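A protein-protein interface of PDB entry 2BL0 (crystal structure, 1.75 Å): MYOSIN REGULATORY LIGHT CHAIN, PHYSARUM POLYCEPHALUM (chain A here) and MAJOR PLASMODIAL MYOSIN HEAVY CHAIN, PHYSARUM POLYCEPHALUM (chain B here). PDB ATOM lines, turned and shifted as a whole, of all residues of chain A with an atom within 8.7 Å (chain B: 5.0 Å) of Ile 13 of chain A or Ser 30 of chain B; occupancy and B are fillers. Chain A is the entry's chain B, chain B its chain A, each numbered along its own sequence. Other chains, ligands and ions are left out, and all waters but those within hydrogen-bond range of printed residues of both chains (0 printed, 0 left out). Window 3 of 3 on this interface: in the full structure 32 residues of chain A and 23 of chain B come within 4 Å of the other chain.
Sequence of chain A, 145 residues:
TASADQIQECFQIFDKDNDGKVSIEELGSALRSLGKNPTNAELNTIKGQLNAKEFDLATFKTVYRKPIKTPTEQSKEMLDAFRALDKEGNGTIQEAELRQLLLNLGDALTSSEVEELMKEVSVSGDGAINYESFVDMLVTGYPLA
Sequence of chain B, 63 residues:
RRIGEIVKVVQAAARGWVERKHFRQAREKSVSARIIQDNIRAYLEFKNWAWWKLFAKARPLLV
Hydrophobic or aromatic side chains of chain A within 4 Å of the printed part of chain B: Ile 13. Of the 10 printed residues of chain B, 4 touch a printed residue of chain A. Printed residues of chain B that touch a printed residue of chain A: Phe 23, Arg 27, Ser 30 and Val 31. Hydrophobic or aromatic side chains of chain B that line the printed part of chain A: Phe 23 and Val 31. Among the printed residues, 7 pairs touch across the chains.
O of Ala 30 of chain A sits at hydrogen-bond distance from SG of Cys 10 of chain A (3.8 Å).
CG2 of Val 31 of chain B touches OE2 of Glu 9 of chain A (3.4 Å). Phe 23 of chain B touches Cys 10 of chain A (CZ to CB, 3.7 Å). Ile 13 of chain A touches Phe 23 of chain B (CD1 to CE1, 3.8 Å). CA of Arg 27 of chain B touches CD1 of Ile 13 of chain A, at 3.8 Å. Ser 30 of chain B touches Ile 13 of chain A. Ser 33 of chain A touches Phe 23 of chain B.
Printed residues of chain B within 4 Å of Cys 10 of chain A: Phe 23. Ile 13 of chain A touches just these residues of chain B: Phe 23 (3.8 Å), Arg 27 (3.8 Å) and Ser 30 (3.8 Å). Of chain A, only Ile 13 comes within 4 Å of Ser 30 of chain B. Of the printed residues of chain A, Val 31 of chain B touches Glu 9. The nearest residue of chain A that does not touch Ser 30 of chain B is Glu 9 of chain A (6.4 Å). The nearest printed residue of chain A that does not touch Arg 27 of chain B is Gln 6 of chain A (6.3 Å).
NE of Arg 27 of chain B is in salt-bridge range of OE1 of Glu 9 of chain A, 3.0 Å away.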
ATOM      1  N   ASP A   5      16.028  12.469 -21.775  1.00  0.00           N
ATOM      2  CA  ASP A   5      16.042  11.122 -21.221  1.00  0.00           C
ATOM      3  C   ASP A   5      14.781  10.390 -21.632  1.00  0.00           C
ATOM      4  O   ASP A   5      14.837   9.211 -21.938  1.00  0.00           O
ATOM      5  CB  ASP A   5      16.172  11.131 -19.689  1.00  0.00           C
ATOM      6  CG  ASP A   5      17.574  11.483 -19.212  1.00  0.00           C
ATOM      7  OD1 ASP A   5      18.557  11.315 -19.970  1.00  0.00           O
ATOM      8  OD2 ASP A   5      17.785  11.939 -18.065  1.00  0.00           O
ATOM      9  N   GLN A   6      13.656  11.093 -21.654  1.00  0.00           N
ATOM     10  CA  GLN A   6      12.387  10.490 -22.041  1.00  0.00           C
ATOM     11  C   GLN A   6      12.384  10.163 -23.527  1.00  0.00           C
ATOM     12  O   GLN A   6      11.835   9.152 -23.933  1.00  0.00           O
ATOM     13  CB  GLN A   6      11.206  11.398 -21.707  1.00  0.00           C
ATOM     14  CG  GLN A   6      10.836  11.435 -20.225  1.00  0.00           C
ATOM     15  CD  GLN A   6       9.791  12.483 -19.920  1.00  0.00           C
ATOM     16  OE1 GLN A   6       9.937  13.630 -20.319  1.00  0.00           O
ATOM     17  NE2 GLN A   6       8.744  12.098 -19.193  1.00  0.00           N
ATOM     18  N   ILE A   7      12.983  11.033 -24.341  1.00  0.00           N
ATOM     19  CA  ILE A   7      13.082  10.767 -25.776  1.00  0.00           C
ATOM     20  C   ILE A   7      13.961   9.536 -26.033  1.00  0.00           C
ATOM     21  O   ILE A   7      13.593   8.659 -26.817  1.00  0.00           O
ATOM     22  CB  ILE A   7      13.595  12.018 -26.561  1.00  0.00           C
ATOM     23  CG1 ILE A   7      12.570  13.151 -26.492  1.00  0.00           C
ATOM     24  CG2 ILE A   7      13.816  11.675 -27.997  1.00  0.00           C
ATOM     25  CD1 ILE A   7      13.121  14.528 -26.869  1.00  0.00           C
ATOM     26  N   GLN A   8      15.104   9.451 -25.358  1.00  0.00           N
ATOM     27  CA  GLN A   8      15.962   8.267 -25.502  1.00  0.00           C
ATOM     28  C   GLN A   8      15.251   6.979 -25.075  1.00  0.00           C
ATOM     29  O   GLN A   8      15.340   5.955 -25.739  1.00  0.00           O
ATOM     30  CB  GLN A   8      17.248   8.430 -24.690  1.00  0.00           C
ATOM     31  CG  GLN A   8      18.159   7.205 -24.736  1.00  0.00           C
ATOM     32  CD  GLN A   8      19.454   7.428 -23.985  1.00  0.00           C
ATOM     33  OE1 GLN A   8      20.534   7.171 -24.511  1.00  0.00           O
ATOM     34  NE2 GLN A   8      19.347   7.903 -22.762  1.00  0.00           N
ATOM     35  N   GLU A   9      14.551   7.038 -23.951  1.00  0.00           N
ATOM     36  CA  GLU A   9      13.842   5.892 -23.413  1.00  0.00           C
ATOM     37  C   GLU A   9      12.815   5.388 -24.404  1.00  0.00           C
ATOM     38  O   GLU A   9      12.670   4.186 -24.625  1.00  0.00           O
ATOM     39  CB  GLU A   9      13.129   6.298 -22.113  1.00  0.00           C
ATOM     40  CG  GLU A   9      12.342   5.192 -21.426  1.00  0.00           C
ATOM     41  CD  GLU A   9      11.649   5.651 -20.157  1.00  0.00           C
ATOM     42  OE1 GLU A   9      11.056   6.749 -20.140  1.00  0.00           O
ATOM     43  OE2 GLU A   9      11.712   4.909 -19.168  1.00  0.00           O
ATOM     44  N   CYS A  10      12.059   6.326 -24.960  1.00  0.00           N
ATOM     45  CA  CYS A  10      11.060   5.997 -25.946  1.00  0.00           C
ATOM     46  C   CYS A  10      11.690   5.339 -27.154  1.00  0.00           C
ATOM     47  O   CYS A  10      11.230   4.283 -27.572  1.00  0.00           O
ATOM     48  CB  CYS A  10      10.275   7.247 -26.345  1.00  0.00           C
ATOM     49  SG  CYS A  10       9.157   7.029 -27.769  1.00  0.00           S
ATOM     50  N   PHE A  11      12.766   5.926 -27.681  1.00  0.00           N
ATOM     51  CA  PHE A  11      13.446   5.372 -28.844  1.00  0.00           C
ATOM     52  C   PHE A  11      13.897   3.938 -28.575  1.00  0.00           C
ATOM     53  O   PHE A  11      13.684   3.056 -29.399  1.00  0.00           O
ATOM     54  CB  PHE A  11      14.636   6.240 -29.246  1.00  0.00           C
ATOM     55  CG  PHE A  11      15.336   5.764 -30.495  1.00  0.00           C
ATOM     56  CD1 PHE A  11      14.943   6.233 -31.757  1.00  0.00           C
ATOM     57  CD2 PHE A  11      16.378   4.873 -30.412  1.00  0.00           C
ATOM     58  CE1 PHE A  11      15.570   5.791 -32.903  1.00  0.00           C
ATOM     59  CE2 PHE A  11      17.011   4.435 -31.537  1.00  0.00           C
ATOM     60  CZ  PHE A  11      16.620   4.891 -32.789  1.00  0.00           C
ATOM     61  N   GLN A  12      14.492   3.716 -27.415  1.00  0.00           N
ATOM     62  CA  GLN A  12      15.006   2.401 -27.065  1.00  0.00           C
ATOM     63  C   GLN A  12      13.886   1.366 -26.986  1.00  0.00           C
ATOM     64  O   GLN A  12      14.089   0.204 -27.313  1.00  0.00           O
ATOM     65  CB  GLN A  12      15.777   2.449 -25.739  1.00  0.00           C
ATOM     66  CG  GLN A  12      17.039   3.256 -25.850  1.00  0.00           C
ATOM     67  CD  GLN A  12      17.839   3.323 -24.568  1.00  0.00           C
ATOM     68  OE1 GLN A  12      19.052   3.488 -24.624  1.00  0.00           O
ATOM     69  NE2 GLN A  12      17.176   3.202 -23.421  1.00  0.00           N
ATOM     70  N   ILE A  13      12.701   1.784 -26.551  1.00  0.00           N
ATOM     71  CA  ILE A  13      11.553   0.886 -26.490  1.00  0.00           C
ATOM     72  C   ILE A  13      11.114   0.457 -27.893  1.00  0.00           C
ATOM     73  O   ILE A  13      10.804  -0.709 -28.110  1.00  0.00           O
ATOM     74  CB  ILE A  13      10.400   1.527 -25.666  1.00  0.00           C
ATOM     75  CG1 ILE A  13      10.736   1.479 -24.166  1.00  0.00           C
ATOM     76  CG2 ILE A  13       9.078   0.827 -25.904  1.00  0.00           C
ATOM     77  CD1 ILE A  13       9.889   2.387 -23.345  1.00  0.00           C
ATOM     78  N   PHE A  14      11.127   1.394 -28.841  1.00  0.00           N
ATOM     79  CA  PHE A  14      10.812   1.108 -30.232  1.00  0.00           C
ATOM     80  C   PHE A  14      11.903   0.291 -30.926  1.00  0.00           C
ATOM     81  O   PHE A  14      11.606  -0.478 -31.834  1.00  0.00           O
ATOM     82  CB  PHE A  14      10.546   2.396 -31.011  1.00  0.00           C
ATOM     83  CG  PHE A  14       9.139   2.902 -30.877  1.00  0.00           C
ATOM     84  CD1 PHE A  14       8.739   3.633 -29.772  1.00  0.00           C
ATOM     85  CD2 PHE A  14       8.208   2.635 -31.867  1.00  0.00           C
ATOM     86  CE1 PHE A  14       7.414   4.079 -29.639  1.00  0.00           C
ATOM     87  CE2 PHE A  14       6.910   3.056 -31.746  1.00  0.00           C
ATOM     88  CZ  PHE A  14       6.498   3.780 -30.640  1.00  0.00           C
ATOM     89  N   ASP A  15      13.152   0.459 -30.496  1.00  0.00           N
ATOM     90  CA  ASP A  15      14.302  -0.216 -31.114  1.00  0.00           C
ATOM     91  C   ASP A  15      14.457  -1.572 -30.430  1.00  0.00           C
ATOM     92  O   ASP A  15      15.364  -1.790 -29.620  1.00  0.00           O
ATOM     93  CB  ASP A  15      15.556   0.636 -30.952  1.00  0.00           C
ATOM     94  CG  ASP A  15      16.783   0.027 -31.601  1.00  0.00           C
ATOM     95  OD1 ASP A  15      16.646  -0.808 -32.524  1.00  0.00           O
ATOM     96  OD2 ASP A  15      17.944   0.370 -31.256  1.00  0.00           O
ATOM     97  N   LYS A  16      13.559  -2.482 -30.774  1.00  0.00           N
ATOM     98  CA  LYS A  16      13.471  -3.765 -30.072  1.00  0.00           C
ATOM     99  C   LYS A  16      14.737  -4.621 -30.221  1.00  0.00           C
ATOM    100  O   LYS A  16      15.115  -5.348 -29.284  1.00  0.00           O
ATOM    101  CB  LYS A  16      12.224  -4.517 -30.540  1.00  0.00           C
ATOM    102  CG  LYS A  16      10.919  -3.893 -29.997  1.00  0.00           C
ATOM    103  CD  LYS A  16       9.722  -4.828 -30.171  1.00  0.00           C
ATOM    104  CE  LYS A  16       8.381  -4.090 -30.009  1.00  0.00           C
ATOM    105  NZ  LYS A  16       7.558  -4.088 -31.264  1.00  0.00           N
ATOM    106  N   ASP A  17      15.404  -4.514 -31.370  1.00  0.00           N
ATOM    107  CA  ASP A  17      16.615  -5.315 -31.644  1.00  0.00           C
ATOM    108  C   ASP A  17      17.934  -4.578 -31.317  1.00  0.00           C
ATOM    109  O   ASP A  17      19.025  -5.110 -31.526  1.00  0.00           O
ATOM    110  CB  ASP A  17      16.600  -5.878 -33.080  1.00  0.00           C
ATOM    111  CG  ASP A  17      16.789  -4.824 -34.147  1.00  0.00           C
ATOM    112  OD1 ASP A  17      16.646  -3.632 -33.844  1.00  0.00           O
ATOM    113  OD2 ASP A  17      17.067  -5.087 -35.340  1.00  0.00           O
ATOM    114  N   ASN A  18      17.826  -3.360 -30.783  1.00  0.00           N
ATOM    115  CA  ASN A  18      18.972  -2.651 -30.199  1.00  0.00           C
ATOM    116  C   ASN A  18      20.090  -2.332 -31.191  1.00  0.00           C
ATOM    117  O   ASN A  18      21.265  -2.331 -30.828  1.00  0.00           O
ATOM    118  CB  ASN A  18      19.552  -3.425 -29.005  1.00  0.00           C
ATOM    119  CG  ASN A  18      18.521  -3.702 -27.937  1.00  0.00           C
ATOM    120  OD1 ASN A  18      18.214  -4.855 -27.642  1.00  0.00           O
ATOM    121  ND2 ASN A  18      17.989  -2.653 -27.348  1.00  0.00           N
ATOM    122  N   LYS A  21      18.489   1.803 -34.753  1.00  0.00           N
ATOM    123  CA  LYS A  21      17.606   2.234 -35.844  1.00  0.00           C
ATOM    124  C   LYS A  21      16.163   1.813 -35.610  1.00  0.00           C
ATOM    125  O   LYS A  21      15.884   0.738 -35.102  1.00  0.00           O
ATOM    126  CB  LYS A  21      18.068   1.665 -37.185  1.00  0.00           C
ATOM    127  CG  LYS A  21      19.443   2.119 -37.616  1.00  0.00           C
ATOM    128  CD  LYS A  21      19.513   3.598 -37.946  1.00  0.00           C
ATOM    129  CE  LYS A  21      20.089   3.848 -39.334  1.00  0.00           C
ATOM    130  NZ  LYS A  21      21.196   2.953 -39.664  1.00  0.00           N
ATOM    131  N   VAL A  22      15.235   2.674 -36.006  1.00  0.00           N
ATOM    132  CA  VAL A  22      13.810   2.379 -35.909  1.00  0.00           C
ATOM    133  C   VAL A  22      13.219   2.629 -37.287  1.00  0.00           C
ATOM    134  O   VAL A  22      13.604   3.584 -37.957  1.00  0.00           O
ATOM    135  CB  VAL A  22      13.126   3.238 -34.811  1.00  0.00           C
ATOM    136  CG1 VAL A  22      11.645   3.134 -34.898  1.00  0.00           C
ATOM    137  CG2 VAL A  22      13.616   2.813 -33.418  1.00  0.00           C
ATOM    138  N   ALA A  30       6.037   6.760 -32.620  1.00  0.00           N
ATOM    139  CA  ALA A  30       7.034   7.209 -31.648  1.00  0.00           C
ATOM    140  C   ALA A  30       6.821   8.678 -31.253  1.00  0.00           C
ATOM    141  O   ALA A  30       6.883   9.015 -30.061  1.00  0.00           O
ATOM    142  CB  ALA A  30       8.447   6.966 -32.202  1.00  0.00           C
ATOM    143  N   SER A  33       3.705   8.826 -29.163  1.00  0.00           N
ATOM    144  CA  SER A  33       3.950   8.238 -27.858  1.00  0.00           C
ATOM    145  C   SER A  33       4.375   9.293 -26.848  1.00  0.00           C
ATOM    146  O   SER A  33       4.064   9.159 -25.661  1.00  0.00           O
ATOM    147  CB  SER A  33       5.011   7.126 -27.932  1.00  0.00           C
ATOM    148  OG  SER A  33       4.513   5.994 -28.638  1.00  0.00           O
ATOM    149  N   LEU A  34       5.087  10.314 -27.327  1.00  0.00           N
ATOM    150  CA  LEU A  34       5.636  11.397 -26.519  1.00  0.00           C
ATOM    151  C   LEU A  34       4.842  12.727 -26.600  1.00  0.00           C
ATOM    152  O   LEU A  34       5.350  13.798 -26.246  1.00  0.00           O
ATOM    153  CB  LEU A  34       7.093  11.637 -26.898  1.00  0.00           C
ATOM    154  CG  LEU A  34       8.044  10.476 -26.551  1.00  0.00           C
ATOM    155  CD1 LEU A  34       9.452  10.848 -26.928  1.00  0.00           C
ATOM    156  CD2 LEU A  34       7.963  10.111 -25.093  1.00  0.00           C
ATOM    157  N   PHE A  60      15.439  11.361 -34.392  1.00  0.00           N
ATOM    158  CA  PHE A  60      14.200  11.360 -33.650  1.00  0.00           C
ATOM    159  C   PHE A  60      14.124  12.600 -32.781  1.00  0.00           C
ATOM    160  O   PHE A  60      13.085  13.244 -32.730  1.00  0.00           O
ATOM    161  CB  PHE A  60      14.122  10.110 -32.785  1.00  0.00           C
ATOM    162  CG  PHE A  60      12.840   9.957 -32.018  1.00  0.00           C
ATOM    163  CD1 PHE A  60      11.591  10.114 -32.636  1.00  0.00           C
ATOM    164  CD2 PHE A  60      12.870   9.576 -30.696  1.00  0.00           C
ATOM    165  CE1 PHE A  60      10.429   9.909 -31.909  1.00  0.00           C
ATOM    166  CE2 PHE A  60      11.708   9.381 -29.987  1.00  0.00           C
ATOM    167  CZ  PHE A  60      10.494   9.543 -30.599  1.00  0.00           C
ATOM    168  N   PHE B  23       1.916   3.192 -25.338  1.00  0.00           N
ATOM    169  CA  PHE B  23       3.246   3.511 -24.834  1.00  0.00           C
ATOM    170  C   PHE B  23       3.296   3.431 -23.315  1.00  0.00           C
ATOM    171  O   PHE B  23       4.273   2.939 -22.739  1.00  0.00           O
ATOM    172  CB  PHE B  23       3.718   4.889 -25.307  1.00  0.00           C
ATOM    173  CG  PHE B  23       5.127   5.168 -24.923  1.00  0.00           C
ATOM    174  CD1 PHE B  23       6.148   4.429 -25.493  1.00  0.00           C
ATOM    175  CD2 PHE B  23       5.437   6.110 -23.951  1.00  0.00           C
ATOM    176  CE1 PHE B  23       7.467   4.647 -25.123  1.00  0.00           C
ATOM    177  CE2 PHE B  23       6.755   6.332 -23.583  1.00  0.00           C
ATOM    178  CZ  PHE B  23       7.765   5.601 -24.177  1.00  0.00           C
ATOM    179  N   ALA B  26       3.782  -0.251 -22.614  1.00  0.00           N
ATOM    180  CA  ALA B  26       5.086  -0.727 -23.052  1.00  0.00           C
ATOM    181  C   ALA B  26       6.196  -0.190 -22.165  1.00  0.00           C
ATOM    182  O   ALA B  26       7.139  -0.908 -21.849  1.00  0.00           O
ATOM    183  CB  ALA B  26       5.335  -0.332 -24.475  1.00  0.00           C
ATOM    184  N   ARG B  27       6.084   1.080 -21.774  1.00  0.00           N
ATOM    185  CA  ARG B  27       7.069   1.714 -20.889  1.00  0.00           C
ATOM    186  C   ARG B  27       7.028   1.110 -19.490  1.00  0.00           C
ATOM    187  O   ARG B  27       8.067   0.862 -18.896  1.00  0.00           O
ATOM    188  CB  ARG B  27       6.842   3.228 -20.789  1.00  0.00           C
ATOM    189  CG  ARG B  27       7.954   3.923 -20.055  1.00  0.00           C
ATOM    190  CD  ARG B  27       7.796   5.424 -19.850  1.00  0.00           C
ATOM    191  NE  ARG B  27       8.555   5.821 -18.662  1.00  0.00           N
ATOM    192  CZ  ARG B  27       8.144   5.621 -17.414  1.00  0.00           C
ATOM    193  NH1 ARG B  27       6.965   5.063 -17.169  1.00  0.00           N
ATOM    194  NH2 ARG B  27       8.908   6.003 -16.404  1.00  0.00           N
ATOM    195  N   GLU B  28       5.833   0.845 -18.975  1.00  0.00           N
ATOM    196  CA  GLU B  28       5.723   0.272 -17.633  1.00  0.00           C
ATOM    197  C   GLU B  28       6.419  -1.073 -17.604  1.00  0.00           C
ATOM    198  O   GLU B  28       7.195  -1.355 -16.684  1.00  0.00           O
ATOM    199  CB  GLU B  28       4.259   0.176 -17.181  1.00  0.00           C
ATOM    200  CG  GLU B  28       3.693   1.516 -16.680  1.00  0.00           C
ATOM    201  CD  GLU B  28       2.181   1.530 -16.468  1.00  0.00           C
ATOM    202  OE1 GLU B  28       1.475   0.594 -16.912  1.00  0.00           O
ATOM    203  OE2 GLU B  28       1.683   2.514 -15.871  1.00  0.00           O
ATOM    204  N   LYS B  29       6.186  -1.883 -18.635  1.00  0.00           N
ATOM    205  CA  LYS B  29       6.817  -3.192 -18.764  1.00  0.00           C
ATOM    206  C   LYS B  29       8.329  -3.073 -18.877  1.00  0.00           C
ATOM    207  O   LYS B  29       9.052  -3.824 -18.217  1.00  0.00           O
ATOM    208  CB  LYS B  29       6.240  -3.950 -19.973  1.00  0.00           C
ATOM    209  CG  LYS B  29       6.669  -5.385 -20.114  1.00  0.00           C
ATOM    210  CD  LYS B  29       5.946  -6.103 -21.272  1.00  0.00           C
ATOM    211  CE  LYS B  29       6.153  -7.624 -21.250  1.00  0.00           C
ATOM    212  NZ  LYS B  29       6.847  -8.200 -22.433  1.00  0.00           N
ATOM    213  N   SER B  30       8.820  -2.132 -19.690  1.00  0.00           N
ATOM    214  CA  SER B  30      10.270  -2.003 -19.891  1.00  0.00           C
ATOM    215  C   SER B  30      10.984  -1.472 -18.645  1.00  0.00           C
ATOM    216  O   SER B  30      12.100  -1.904 -18.324  1.00  0.00           O
ATOM    217  CB  SER B  30      10.608  -1.105 -21.090  1.00  0.00           C
ATOM    218  OG  SER B  30      10.547  -1.866 -22.305  1.00  0.00           O
ATOM    219  N   VAL B  31      10.348  -0.539 -17.947  1.00  0.00           N
ATOM    220  CA  VAL B  31      10.941   0.057 -16.747  1.00  0.00           C
ATOM    221  C   VAL B  31      11.033  -1.002 -15.647  1.00  0.00           C
ATOM    222  O   VAL B  31      12.054  -1.107 -14.957  1.00  0.00           O
ATOM    223  CB  VAL B  31      10.133   1.303 -16.274  1.00  0.00           C
ATOM    224  CG1 VAL B  31      10.418   1.658 -14.804  1.00  0.00           C
ATOM    225  CG2 VAL B  31      10.435   2.494 -17.167  1.00  0.00           C
ATOM    226  N   SER B  32       9.977  -1.788 -15.504  1.00  0.00           N
ATOM    227  CA  SER B  32       9.932  -2.862 -14.507  1.00  0.00           C
ATOM    228  C   SER B  32      10.933  -3.962 -14.808  1.00  0.00           C
ATOM    229  O   SER B  32      11.604  -4.448 -13.903  1.00  0.00           O
ATOM    230  CB  SER B  32       8.531  -3.436 -14.396  1.00  0.00           C
ATOM    231  OG  SER B  32       7.673  -2.501 -13.780  1.00  0.00           O
ATOM    232  N   ALA B  33      11.035  -4.351 -16.075  1.00  0.00           N
ATOM    233  CA  ALA B  33      11.997  -5.345 -16.506  1.00  0.00           C
ATOM    234  C   ALA B  33      13.390  -4.850 -16.188  1.00  0.00           C
ATOM    235  O   ALA B  33      14.214  -5.596 -15.715  1.00  0.00           O
ATOM    236  CB  ALA B  33      11.885  -5.597 -17.980  1.00  0.00           C
ATOM    237  N   ARG B  34      13.655  -3.576 -16.456  1.00  0.00           N
ATOM    238  CA  ARG B  34      14.955  -3.009 -16.154  1.00  0.00           C
ATOM    239  C   ARG B  34      15.336  -3.058 -14.673  1.00  0.00           C
ATOM    240  O   ARG B  34      16.467  -3.394 -14.326  1.00  0.00           O
ATOM    241  CB  ARG B  34      15.050  -1.579 -16.679  1.00  0.00           C
ATOM    242  CG  ARG B  34      16.432  -0.972 -16.506  1.00  0.00           C
ATOM    243  CD  ARG B  34      17.514  -1.638 -17.330  1.00  0.00           C
ATOM    244  NE  ARG B  34      18.841  -1.144 -16.986  1.00  0.00           N
ATOM    245  CZ  ARG B  34      19.488  -0.186 -17.647  1.00  0.00           C
ATOM    246  NH1 ARG B  34      18.971   0.365 -18.742  1.00  0.00           N
ATOM    247  NH2 ARG B  34      20.691   0.191 -17.225  1.00  0.00           N
